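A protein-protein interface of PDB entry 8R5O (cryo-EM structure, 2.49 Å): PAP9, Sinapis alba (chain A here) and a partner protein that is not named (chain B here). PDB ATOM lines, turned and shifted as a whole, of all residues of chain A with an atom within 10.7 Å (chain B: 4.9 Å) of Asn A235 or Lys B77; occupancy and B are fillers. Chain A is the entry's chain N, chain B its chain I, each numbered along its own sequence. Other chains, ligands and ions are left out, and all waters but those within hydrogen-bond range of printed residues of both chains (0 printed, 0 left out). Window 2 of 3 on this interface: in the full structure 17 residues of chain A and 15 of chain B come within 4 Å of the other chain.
OH of Tyr A230 lies within hydrogen-bond range of NE2 of His B78 (2.6 Å). The side-chain carboxylate of Glu A234 is in salt-bridge range of the guanidinium group of Arg B69, 3.1 Å away.
The guanidinium group (NH1) of Arg B69 lies within salt-bridge range of the side-chain carboxylate (OE1) of Glu B72, 3.2 Å away. The side-chain carboxylate of Glu A234 lies within salt-bridge range of the guanidinium group of Arg A236, 3.8 Å away. The backbone NH of His B78 is in hydrogen-bond range of the backbone carbonyl oxygen of Val B73, at 3.0 Å.
CE1 of His B78 touches OE2 of Glu A226, at 3.9 Å. Val B73 touches Tyr A230 (CG1 to OH, 3.2 Å). Asn A235 touches Lys B77. NE2 of His B78 touches CB of Asn A235, at 3.6 Å.
Lys B77 touches one residue of chain A. His B78 touches just these residues of chain A: Glu A226, Tyr A230 and Asn A235. No residue of chain A comes within 4 Å of Gly B81. Of the printed residues of chain B, Glu A226 touches His B78. Printed residues of chain B within 4 Å of Tyr A230: Val B73 and His B78. Printed residues of chain A within 4 Å of Arg B69: Glu A234. Of the printed residues of chain B, Glu A234 touches Arg B69. His B74 touches none of the printed residues of chain A. Ile A241 touches none of the printed residues of chain B. The nearest residue of chain B that does not touch Asn A235 is Val B73 (4.1 Å). The nearest printed residue of chain B that does not touch Glu A226 is His B74 (8.1 Å).
Hydrophobic or aromatic side chains of chain B that line the printed part of chain A: Val B73 and His B78. Along chain B the printed residues that touch a printed residue of chain A span positions 69 to 78. Hydrophobic or aromatic side chains of chain A within 4 Å of the printed part of chain B: Tyr A230. Among the printed residues, 6 pairs touch across the chains.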
ATOM      1  N   ALA A 165      -6.788   8.672 -20.976  1.00  0.00           N
ATOM      2  CA  ALA A 165      -6.106   7.562 -20.325  1.00  0.00           C
ATOM      3  C   ALA A 165      -5.827   7.857 -18.857  1.00  0.00           C
ATOM      4  O   ALA A 165      -5.800   6.935 -18.034  1.00  0.00           O
ATOM      5  CB  ALA A 165      -4.809   7.234 -21.063  1.00  0.00           C
ATOM      6  N   ALA A 166      -5.619   9.129 -18.511  1.00  0.00           N
ATOM      7  CA  ALA A 166      -5.343   9.485 -17.122  1.00  0.00           C
ATOM      8  C   ALA A 166      -6.599   9.413 -16.264  1.00  0.00           C
ATOM      9  O   ALA A 166      -6.542   8.980 -15.108  1.00  0.00           O
ATOM     10  CB  ALA A 166      -4.728  10.879 -17.053  1.00  0.00           C
ATOM     11  N   ASN A 168      -9.269   7.563 -16.669  1.00  0.00           N
ATOM     12  CA  ASN A 168      -9.952   6.274 -16.661  1.00  0.00           C
ATOM     13  C   ASN A 168      -9.822   5.653 -15.274  1.00  0.00           C
ATOM     14  O   ASN A 168      -8.753   5.159 -14.904  1.00  0.00           O
ATOM     15  CB  ASN A 168      -9.365   5.364 -17.735  1.00  0.00           C
ATOM     16  CG  ASN A 168     -10.295   4.228 -18.114  1.00  0.00           C
ATOM     17  OD1 ASN A 168     -11.461   4.207 -17.724  1.00  0.00           O
ATOM     18  ND2 ASN A 168      -9.783   3.282 -18.891  1.00  0.00           N
ATOM     19  N   GLY A 170     -10.004   3.201 -12.207  1.00  0.00           N
ATOM     20  CA  GLY A 170      -9.930   1.765 -12.028  1.00  0.00           C
ATOM     21  C   GLY A 170      -9.214   1.064 -13.163  1.00  0.00           C
ATOM     22  O   GLY A 170      -8.372   1.663 -13.839  1.00  0.00           O
ATOM     23  N   THR A 224      -4.450   0.411 -19.122  1.00  0.00           N
ATOM     24  CA  THR A 224      -4.420   1.190 -17.891  1.00  0.00           C
ATOM     25  C   THR A 224      -4.737   0.351 -16.661  1.00  0.00           C
ATOM     26  O   THR A 224      -4.966   0.913 -15.585  1.00  0.00           O
ATOM     27  CB  THR A 224      -5.377   2.381 -17.978  1.00  0.00           C
ATOM     28  OG1 THR A 224      -6.611   1.972 -18.579  1.00  0.00           O
ATOM     29  CG2 THR A 224      -4.759   3.501 -18.801  1.00  0.00           C
ATOM     30  N   TRP A 225      -4.764  -0.973 -16.790  1.00  0.00           N
ATOM     31  CA  TRP A 225      -4.715  -1.823 -15.611  1.00  0.00           C
ATOM     32  C   TRP A 225      -3.407  -1.566 -14.876  1.00  0.00           C
ATOM     33  O   TRP A 225      -2.363  -1.351 -15.496  1.00  0.00           O
ATOM     34  CB  TRP A 225      -4.821  -3.300 -15.997  1.00  0.00           C
ATOM     35  CG  TRP A 225      -6.193  -3.752 -16.414  1.00  0.00           C
ATOM     36  CD1 TRP A 225      -6.929  -3.284 -17.460  1.00  0.00           C
ATOM     37  CD2 TRP A 225      -6.972  -4.790 -15.809  1.00  0.00           C
ATOM     38  NE1 TRP A 225      -8.124  -3.952 -17.537  1.00  0.00           N
ATOM     39  CE2 TRP A 225      -8.177  -4.883 -16.534  1.00  0.00           C
ATOM     40  CE3 TRP A 225      -6.775  -5.642 -14.719  1.00  0.00           C
ATOM     41  CZ2 TRP A 225      -9.176  -5.795 -16.204  1.00  0.00           C
ATOM     42  CZ3 TRP A 225      -7.767  -6.544 -14.394  1.00  0.00           C
ATOM     43  CH2 TRP A 225      -8.953  -6.615 -15.134  1.00  0.00           C
ATOM     44  N   GLU A 226      -3.468  -1.576 -13.544  1.00  0.00           N
ATOM     45  CA  GLU A 226      -2.299  -1.197 -12.761  1.00  0.00           C
ATOM     46  C   GLU A 226      -1.138  -2.166 -12.955  1.00  0.00           C
ATOM     47  O   GLU A 226       0.023  -1.768 -12.817  1.00  0.00           O
ATOM     48  CB  GLU A 226      -2.674  -1.080 -11.284  1.00  0.00           C
ATOM     49  CG  GLU A 226      -3.492   0.165 -10.979  1.00  0.00           C
ATOM     50  CD  GLU A 226      -3.948   0.244  -9.538  1.00  0.00           C
ATOM     51  OE1 GLU A 226      -4.277  -0.808  -8.954  1.00  0.00           O
ATOM     52  OE2 GLU A 226      -3.977   1.364  -8.988  1.00  0.00           O
ATOM     53  N   HIS A 227      -1.418  -3.426 -13.293  1.00  0.00           N
ATOM     54  CA  HIS A 227      -0.337  -4.380 -13.516  1.00  0.00           C
ATOM     55  C   HIS A 227       0.507  -4.034 -14.736  1.00  0.00           C
ATOM     56  O   HIS A 227       1.622  -4.547 -14.869  1.00  0.00           O
ATOM     57  CB  HIS A 227      -0.888  -5.804 -13.650  1.00  0.00           C
ATOM     58  CG  HIS A 227      -1.779  -6.015 -14.838  1.00  0.00           C
ATOM     59  ND1 HIS A 227      -3.093  -6.412 -14.717  1.00  0.00           N
ATOM     60  CD2 HIS A 227      -1.540  -5.911 -16.166  1.00  0.00           C
ATOM     61  CE1 HIS A 227      -3.627  -6.531 -15.918  1.00  0.00           C
ATOM     62  NE2 HIS A 227      -2.707  -6.230 -16.815  1.00  0.00           N
ATOM     63  N   ALA A 228       0.003  -3.182 -15.629  1.00  0.00           N
ATOM     64  CA  ALA A 228       0.747  -2.831 -16.832  1.00  0.00           C
ATOM     65  C   ALA A 228       1.893  -1.868 -16.557  1.00  0.00           C
ATOM     66  O   ALA A 228       2.834  -1.808 -17.354  1.00  0.00           O
ATOM     67  CB  ALA A 228      -0.196  -2.230 -17.875  1.00  0.00           C
ATOM     68  N   TYR A 229       1.842  -1.113 -15.459  1.00  0.00           N
ATOM     69  CA  TYR A 229       2.855  -0.098 -15.209  1.00  0.00           C
ATOM     70  C   TYR A 229       3.348  -0.025 -13.771  1.00  0.00           C
ATOM     71  O   TYR A 229       4.243   0.779 -13.496  1.00  0.00           O
ATOM     72  CB  TYR A 229       2.327   1.288 -15.617  1.00  0.00           C
ATOM     73  CG  TYR A 229       1.098   1.737 -14.854  1.00  0.00           C
ATOM     74  CD1 TYR A 229       1.212   2.435 -13.659  1.00  0.00           C
ATOM     75  CD2 TYR A 229      -0.175   1.471 -15.334  1.00  0.00           C
ATOM     76  CE1 TYR A 229       0.094   2.847 -12.961  1.00  0.00           C
ATOM     77  CE2 TYR A 229      -1.298   1.880 -14.644  1.00  0.00           C
ATOM     78  CZ  TYR A 229      -1.158   2.567 -13.459  1.00  0.00           C
ATOM     79  OH  TYR A 229      -2.275   2.977 -12.771  1.00  0.00           O
ATOM     80  N   TYR A 230       2.809  -0.821 -12.847  1.00  0.00           N
ATOM     81  CA  TYR A 230       3.125  -0.608 -11.439  1.00  0.00           C
ATOM     82  C   TYR A 230       4.560  -0.992 -11.105  1.00  0.00           C
ATOM     83  O   TYR A 230       5.160  -0.402 -10.200  1.00  0.00           O
ATOM     84  CB  TYR A 230       2.151  -1.375 -10.548  1.00  0.00           C
ATOM     85  CG  TYR A 230       1.776  -0.604  -9.307  1.00  0.00           C
ATOM     86  CD1 TYR A 230       0.856   0.432  -9.368  1.00  0.00           C
ATOM     87  CD2 TYR A 230       2.352  -0.896  -8.080  1.00  0.00           C
ATOM     88  CE1 TYR A 230       0.515   1.151  -8.244  1.00  0.00           C
ATOM     89  CE2 TYR A 230       2.016  -0.184  -6.948  1.00  0.00           C
ATOM     90  CZ  TYR A 230       1.096   0.838  -7.036  1.00  0.00           C
ATOM     91  OH  TYR A 230       0.753   1.552  -5.913  1.00  0.00           O
ATOM     92  N   LEU A 231       5.128  -1.972 -11.809  1.00  0.00           N
ATOM     93  CA  LEU A 231       6.510  -2.353 -11.544  1.00  0.00           C
ATOM     94  C   LEU A 231       7.505  -1.335 -12.082  1.00  0.00           C
ATOM     95  O   LEU A 231       8.661  -1.330 -11.647  1.00  0.00           O
ATOM     96  CB  LEU A 231       6.800  -3.732 -12.137  1.00  0.00           C
ATOM     97  CG  LEU A 231       5.970  -4.890 -11.582  1.00  0.00           C
ATOM     98  CD1 LEU A 231       6.378  -6.206 -12.225  1.00  0.00           C
ATOM     99  CD2 LEU A 231       6.097  -4.964 -10.070  1.00  0.00           C
ATOM    100  N   ASP A 232       7.088  -0.475 -13.009  1.00  0.00           N
ATOM    101  CA  ASP A 232       7.980   0.515 -13.599  1.00  0.00           C
ATOM    102  C   ASP A 232       7.711   1.936 -13.128  1.00  0.00           C
ATOM    103  O   ASP A 232       8.644   2.744 -13.081  1.00  0.00           O
ATOM    104  CB  ASP A 232       7.880   0.476 -15.128  1.00  0.00           C
ATOM    105  CG  ASP A 232       8.370  -0.833 -15.710  1.00  0.00           C
ATOM    106  OD1 ASP A 232       9.325  -1.411 -15.153  1.00  0.00           O
ATOM    107  OD2 ASP A 232       7.798  -1.283 -16.722  1.00  0.00           O
ATOM    108  N   PHE A 233       6.466   2.265 -12.782  1.00  0.00           N
ATOM    109  CA  PHE A 233       6.109   3.627 -12.420  1.00  0.00           C
ATOM    110  C   PHE A 233       5.358   3.742 -11.101  1.00  0.00           C
ATOM    111  O   PHE A 233       5.072   4.865 -10.675  1.00  0.00           O
ATOM    112  CB  PHE A 233       5.264   4.272 -13.532  1.00  0.00           C
ATOM    113  CG  PHE A 233       5.957   4.337 -14.861  1.00  0.00           C
ATOM    114  CD1 PHE A 233       6.735   5.429 -15.198  1.00  0.00           C
ATOM    115  CD2 PHE A 233       5.828   3.305 -15.776  1.00  0.00           C
ATOM    116  CE1 PHE A 233       7.374   5.492 -16.420  1.00  0.00           C
ATOM    117  CE2 PHE A 233       6.463   3.363 -16.998  1.00  0.00           C
ATOM    118  CZ  PHE A 233       7.237   4.457 -17.321  1.00  0.00           C
ATOM    119  N   GLU A 234       5.043   2.627 -10.443  1.00  0.00           N
ATOM    120  CA  GLU A 234       4.237   2.605  -9.214  1.00  0.00           C
ATOM    121  C   GLU A 234       2.933   3.355  -9.495  1.00  0.00           C
ATOM    122  O   GLU A 234       2.264   3.050 -10.490  1.00  0.00           O
ATOM    123  CB  GLU A 234       5.066   3.141  -8.052  1.00  0.00           C
ATOM    124  CG  GLU A 234       6.175   2.212  -7.593  1.00  0.00           C
ATOM    125  CD  GLU A 234       7.017   2.815  -6.487  1.00  0.00           C
ATOM    126  OE1 GLU A 234       7.059   4.059  -6.381  1.00  0.00           O
ATOM    127  OE2 GLU A 234       7.636   2.046  -5.721  1.00  0.00           O
ATOM    128  N   ASN A 235       2.546   4.328  -8.672  1.00  0.00           N
ATOM    129  CA  ASN A 235       1.290   5.044  -8.849  1.00  0.00           C
ATOM    130  C   ASN A 235       1.330   6.063  -9.980  1.00  0.00           C
ATOM    131  O   ASN A 235       0.275   6.580 -10.359  1.00  0.00           O
ATOM    132  CB  ASN A 235       0.910   5.750  -7.547  1.00  0.00           C
ATOM    133  CG  ASN A 235       1.906   6.821  -7.155  1.00  0.00           C
ATOM    134  OD1 ASN A 235       3.031   6.523  -6.756  1.00  0.00           O
ATOM    135  ND2 ASN A 235       1.497   8.078  -7.266  1.00  0.00           N
ATOM    136  N   ARG A 236       2.509   6.360 -10.527  1.00  0.00           N
ATOM    137  CA  ARG A 236       2.673   7.429 -11.515  1.00  0.00           C
ATOM    138  C   ARG A 236       2.168   6.951 -12.875  1.00  0.00           C
ATOM    139  O   ARG A 236       2.928   6.566 -13.765  1.00  0.00           O
ATOM    140  CB  ARG A 236       4.128   7.871 -11.579  1.00  0.00           C
ATOM    141  CG  ARG A 236       4.562   8.710 -10.388  1.00  0.00           C
ATOM    142  CD  ARG A 236       6.071   8.860 -10.310  1.00  0.00           C
ATOM    143  NE  ARG A 236       6.705   7.711  -9.675  1.00  0.00           N
ATOM    144  CZ  ARG A 236       7.468   6.828 -10.305  1.00  0.00           C
ATOM    145  NH1 ARG A 236       7.740   6.946 -11.593  1.00  0.00           N
ATOM    146  NH2 ARG A 236       7.974   5.807  -9.622  1.00  0.00           N
ATOM    147  N   ARG A 237       0.842   6.992 -13.037  1.00  0.00           N
ATOM    148  CA  ARG A 237       0.247   6.618 -14.315  1.00  0.00           C
ATOM    149  C   ARG A 237       0.486   7.682 -15.379  1.00  0.00           C
ATOM    150  O   ARG A 237       0.551   7.359 -16.570  1.00  0.00           O
ATOM    151  CB  ARG A 237      -1.252   6.362 -14.150  1.00  0.00           C
ATOM    152  CG  ARG A 237      -1.914   5.808 -15.404  1.00  0.00           C
ATOM    153  CD  ARG A 237      -3.419   6.000 -15.395  1.00  0.00           C
ATOM    154  NE  ARG A 237      -4.109   4.989 -14.602  1.00  0.00           N
ATOM    155  CZ  ARG A 237      -5.426   4.845 -14.561  1.00  0.00           C
ATOM    156  NH1 ARG A 237      -6.227   5.637 -15.252  1.00  0.00           N
ATOM    157  NH2 ARG A 237      -5.950   3.879 -13.814  1.00  0.00           N
ATOM    158  N   ILE A 238       0.622   8.947 -14.973  1.00  0.00           N
ATOM    159  CA  ILE A 238       0.855  10.024 -15.933  1.00  0.00           C
ATOM    160  C   ILE A 238       2.160   9.799 -16.685  1.00  0.00           C
ATOM    161  O   ILE A 238       2.223   9.957 -17.910  1.00  0.00           O
ATOM    162  CB  ILE A 238       0.845  11.387 -15.215  1.00  0.00           C
ATOM    163  CG1 ILE A 238      -0.527  11.662 -14.606  1.00  0.00           C
ATOM    164  CG2 ILE A 238       1.234  12.498 -16.175  1.00  0.00           C
ATOM    165  CD1 ILE A 238      -1.605  11.896 -15.626  1.00  0.00           C
ATOM    166  N   GLU A 239       3.222   9.435 -15.965  1.00  0.00           N
ATOM    167  CA  GLU A 239       4.506   9.180 -16.611  1.00  0.00           C
ATOM    168  C   GLU A 239       4.428   7.977 -17.538  1.00  0.00           C
ATOM    169  O   GLU A 239       5.050   7.967 -18.606  1.00  0.00           O
ATOM    170  CB  GLU A 239       5.593   8.979 -15.557  1.00  0.00           C
ATOM    171  CG  GLU A 239       5.776  10.160 -14.626  1.00  0.00           C
ATOM    172  CD  GLU A 239       6.883   9.938 -13.616  1.00  0.00           C
ATOM    173  OE1 GLU A 239       7.519   8.865 -13.657  1.00  0.00           O
ATOM    174  OE2 GLU A 239       7.116  10.838 -12.783  1.00  0.00           O
ATOM    175  N   TYR A 240       3.681   6.946 -17.138  1.00  0.00           N
ATOM    176  CA  TYR A 240       3.505   5.777 -17.992  1.00  0.00           C
ATOM    177  C   TYR A 240       2.784   6.139 -19.283  1.00  0.00           C
ATOM    178  O   TYR A 240       3.168   5.684 -20.367  1.00  0.00           O
ATOM    179  CB  TYR A 240       2.747   4.695 -17.223  1.00  0.00           C
ATOM    180  CG  TYR A 240       2.112   3.626 -18.077  1.00  0.00           C
ATOM    181  CD1 TYR A 240       2.888   2.698 -18.758  1.00  0.00           C
ATOM    182  CD2 TYR A 240       0.732   3.524 -18.176  1.00  0.00           C
ATOM    183  CE1 TYR A 240       2.306   1.711 -19.526  1.00  0.00           C
ATOM    184  CE2 TYR A 240       0.143   2.541 -18.940  1.00  0.00           C
ATOM    185  CZ  TYR A 240       0.933   1.637 -19.615  1.00  0.00           C
ATOM    186  OH  TYR A 240       0.345   0.657 -20.377  1.00  0.00           O
ATOM    187  N   ILE A 241       1.736   6.959 -19.189  1.00  0.00           N
ATOM    188  CA  ILE A 241       1.009   7.387 -20.381  1.00  0.00           C
ATOM    189  C   ILE A 241       1.895   8.250 -21.270  1.00  0.00           C
ATOM    190  O   ILE A 241       1.906   8.093 -22.496  1.00  0.00           O
ATOM    191  CB  ILE A 241      -0.281   8.121 -19.977  1.00  0.00           C
ATOM    192  CG1 ILE A 241      -1.223   7.170 -19.239  1.00  0.00           C
ATOM    193  CG2 ILE A 241      -0.967   8.711 -21.196  1.00  0.00           C
ATOM    194  CD1 ILE A 241      -2.333   7.869 -18.504  1.00  0.00           C
ATOM    195  N   ARG B  69       7.303  -0.736   2.016  1.00  0.00           N
ATOM    196  CA  ARG B  69       7.199   0.001   0.762  1.00  0.00           C
ATOM    197  C   ARG B  69       5.770  -0.002   0.236  1.00  0.00           C
ATOM    198  O   ARG B  69       5.317   0.982  -0.360  1.00  0.00           O
ATOM    199  CB  ARG B  69       8.156  -0.586  -0.275  1.00  0.00           C
ATOM    200  CG  ARG B  69       8.224   0.214  -1.563  1.00  0.00           C
ATOM    201  CD  ARG B  69       8.500   1.678  -1.271  1.00  0.00           C
ATOM    202  NE  ARG B  69       8.388   2.507  -2.464  1.00  0.00           N
ATOM    203  CZ  ARG B  69       8.427   3.832  -2.458  1.00  0.00           C
ATOM    204  NH1 ARG B  69       8.573   4.514  -1.333  1.00  0.00           N
ATOM    205  NH2 ARG B  69       8.312   4.491  -3.607  1.00  0.00           N
ATOM    206  N   GLU B  72       3.953   2.646   2.212  1.00  0.00           N
ATOM    207  CA  GLU B  72       4.375   3.993   1.842  1.00  0.00           C
ATOM    208  C   GLU B  72       3.693   4.463   0.564  1.00  0.00           C
ATOM    209  O   GLU B  72       3.317   5.633   0.450  1.00  0.00           O
ATOM    210  CB  GLU B  72       5.895   4.043   1.690  1.00  0.00           C
ATOM    211  CG  GLU B  72       6.650   3.917   3.001  1.00  0.00           C
ATOM    212  CD  GLU B  72       8.153   3.852   2.807  1.00  0.00           C
ATOM    213  OE1 GLU B  72       8.597   3.508   1.691  1.00  0.00           O
ATOM    214  OE2 GLU B  72       8.891   4.149   3.770  1.00  0.00           O
ATOM    215  N   VAL B  73       3.539   3.574  -0.415  1.00  0.00           N
ATOM    216  CA  VAL B  73       2.868   3.954  -1.653  1.00  0.00           C
ATOM    217  C   VAL B  73       1.355   3.920  -1.480  1.00  0.00           C
ATOM    218  O   VAL B  73       0.647   4.839  -1.905  1.00  0.00           O
ATOM    219  CB  VAL B  73       3.324   3.046  -2.811  1.00  0.00           C
ATOM    220  CG1 VAL B  73       2.627   3.447  -4.096  1.00  0.00           C
ATOM    221  CG2 VAL B  73       4.830   3.118  -2.975  1.00  0.00           C
ATOM    222  N   HIS B  74       0.835   2.862  -0.853  1.00  0.00           N
ATOM    223  CA  HIS B  74      -0.612   2.705  -0.738  1.00  0.00           C
ATOM    224  C   HIS B  74      -1.223   3.816   0.108  1.00  0.00           C
ATOM    225  O   HIS B  74      -2.229   4.421  -0.276  1.00  0.00           O
ATOM    226  CB  HIS B  74      -0.942   1.331  -0.153  1.00  0.00           C
ATOM    227  CG  HIS B  74      -2.355   0.896  -0.393  1.00  0.00           C
ATOM    228  ND1 HIS B  74      -2.818  -0.351  -0.033  1.00  0.00           N
ATOM    229  CD2 HIS B  74      -3.404   1.537  -0.955  1.00  0.00           C
ATOM    230  CE1 HIS B  74      -4.092  -0.456  -0.363  1.00  0.00           C
ATOM    231  NE2 HIS B  74      -4.471   0.676  -0.924  1.00  0.00           N
ATOM    232  N   TRP B  75      -0.625   4.102   1.264  1.00  0.00           N
ATOM    233  CA  TRP B  75      -1.148   5.158   2.121  1.00  0.00           C
ATOM    234  C   TRP B  75      -0.593   6.524   1.734  1.00  0.00           C
ATOM    235  O   TRP B  75      -1.343   7.500   1.628  1.00  0.00           O
ATOM    236  CB  TRP B  75      -0.838   4.851   3.588  1.00  0.00           C
ATOM    237  CG  TRP B  75      -1.271   5.935   4.527  1.00  0.00           C
ATOM    238  CD1 TRP B  75      -2.515   6.113   5.052  1.00  0.00           C
ATOM    239  CD2 TRP B  75      -0.461   6.996   5.048  1.00  0.00           C
ATOM    240  NE1 TRP B  75      -2.532   7.217   5.867  1.00  0.00           N
ATOM    241  CE2 TRP B  75      -1.283   7.776   5.882  1.00  0.00           C
ATOM    242  CE3 TRP B  75       0.879   7.359   4.888  1.00  0.00           C
ATOM    243  CZ2 TRP B  75      -0.809   8.900   6.556  1.00  0.00           C
ATOM    244  CZ3 TRP B  75       1.346   8.474   5.557  1.00  0.00           C
ATOM    245  CH2 TRP B  75       0.506   9.231   6.380  1.00  0.00           C
ATOM    246  N   GLY B  76       0.721   6.613   1.513  1.00  0.00           N
ATOM    247  CA  GLY B  76       1.353   7.901   1.293  1.00  0.00           C
ATOM    248  C   GLY B  76       1.101   8.512  -0.069  1.00  0.00           C
ATOM    249  O   GLY B  76       1.250   9.728  -0.225  1.00  0.00           O
ATOM    250  N   LYS B  77       0.732   7.703  -1.061  1.00  0.00           N
ATOM    251  CA  LYS B  77       0.469   8.207  -2.405  1.00  0.00           C
ATOM    252  C   LYS B  77      -0.974   8.014  -2.840  1.00  0.00           C
ATOM    253  O   LYS B  77      -1.626   8.983  -3.243  1.00  0.00           O
ATOM    254  CB  LYS B  77       1.406   7.536  -3.422  1.00  0.00           C
ATOM    255  CG  LYS B  77       2.653   8.334  -3.750  1.00  0.00           C
ATOM    256  CD  LYS B  77       3.841   7.877  -2.932  1.00  0.00           C
ATOM    257  CE  LYS B  77       5.093   8.646  -3.318  1.00  0.00           C
ATOM    258  NZ  LYS B  77       6.291   8.145  -2.594  1.00  0.00           N
ATOM    259  N   HIS B  78      -1.494   6.788  -2.775  1.00  0.00           N
ATOM    260  CA  HIS B  78      -2.862   6.539  -3.221  1.00  0.00           C
ATOM    261  C   HIS B  78      -3.872   7.177  -2.277  1.00  0.00           C
ATOM    262  O   HIS B  78      -4.709   7.984  -2.696  1.00  0.00           O
ATOM    263  CB  HIS B  78      -3.113   5.035  -3.342  1.00  0.00           C
ATOM    264  CG  HIS B  78      -2.434   4.400  -4.515  1.00  0.00           C
ATOM    265  ND1 HIS B  78      -2.900   4.533  -5.805  1.00  0.00           N
ATOM    266  CD2 HIS B  78      -1.331   3.619  -4.592  1.00  0.00           C
ATOM    267  CE1 HIS B  78      -2.111   3.867  -6.626  1.00  0.00           C
ATOM    268  NE2 HIS B  78      -1.150   3.303  -5.915  1.00  0.00           N
ATOM    269  N   HIS B  79      -3.807   6.825  -0.991  1.00  0.00           N
ATOM    270  CA  HIS B  79      -4.750   7.377  -0.026  1.00  0.00           C
ATOM    271  C   HIS B  79      -4.601   8.890   0.083  1.00  0.00           C
ATOM    272  O   HIS B  79      -5.598   9.613   0.166  1.00  0.00           O
ATOM    273  CB  HIS B  79      -4.555   6.714   1.337  1.00  0.00           C
ATOM    274  CG  HIS B  79      -5.677   6.965   2.297  1.00  0.00           C
ATOM    275  ND1 HIS B  79      -5.684   6.462   3.578  1.00  0.00           N
ATOM    276  CD2 HIS B  79      -6.830   7.660   2.160  1.00  0.00           C
ATOM    277  CE1 HIS B  79      -6.791   6.839   4.191  1.00  0.00           C
ATOM    278  NE2 HIS B  79      -7.503   7.568   3.351  1.00  0.00           N
ATOM    279  N   ARG B  80      -3.361   9.384   0.078  1.00  0.00           N
ATOM    280  CA  ARG B  80      -3.139  10.827   0.134  1.00  0.00           C
ATOM    281  C   ARG B  80      -3.723  11.525  -1.087  1.00  0.00           C
ATOM    282  O   ARG B  80      -4.321  12.601  -0.970  1.00  0.00           O
ATOM    283  CB  ARG B  80      -1.647  11.123   0.255  1.00  0.00           C
ATOM    284  CG  ARG B  80      -1.318  12.601   0.368  1.00  0.00           C
ATOM    285  CD  ARG B  80       0.180  12.837   0.387  1.00  0.00           C
ATOM    286  NE  ARG B  80       0.841  12.066   1.434  1.00  0.00           N
ATOM    287  CZ  ARG B  80       0.948  12.454   2.696  1.00  0.00           C
ATOM    288  NH1 ARG B  80       0.444  13.605   3.108  1.00  0.00           N
ATOM    289  NH2 ARG B  80       1.572  11.667   3.566  1.00  0.00           N
ATOM    290  N   GLY B  81      -3.555  10.931  -2.270  1.00  0.00           N
ATOM    291  CA  GLY B  81      -4.097  11.536  -3.475  1.00  0.00           C
ATOM    292  C   GLY B  81      -5.611  11.629  -3.455  1.00  0.00           C
ATOM    293  O   GLY B  81      -6.189  12.605  -3.940  1.00  0.00           O
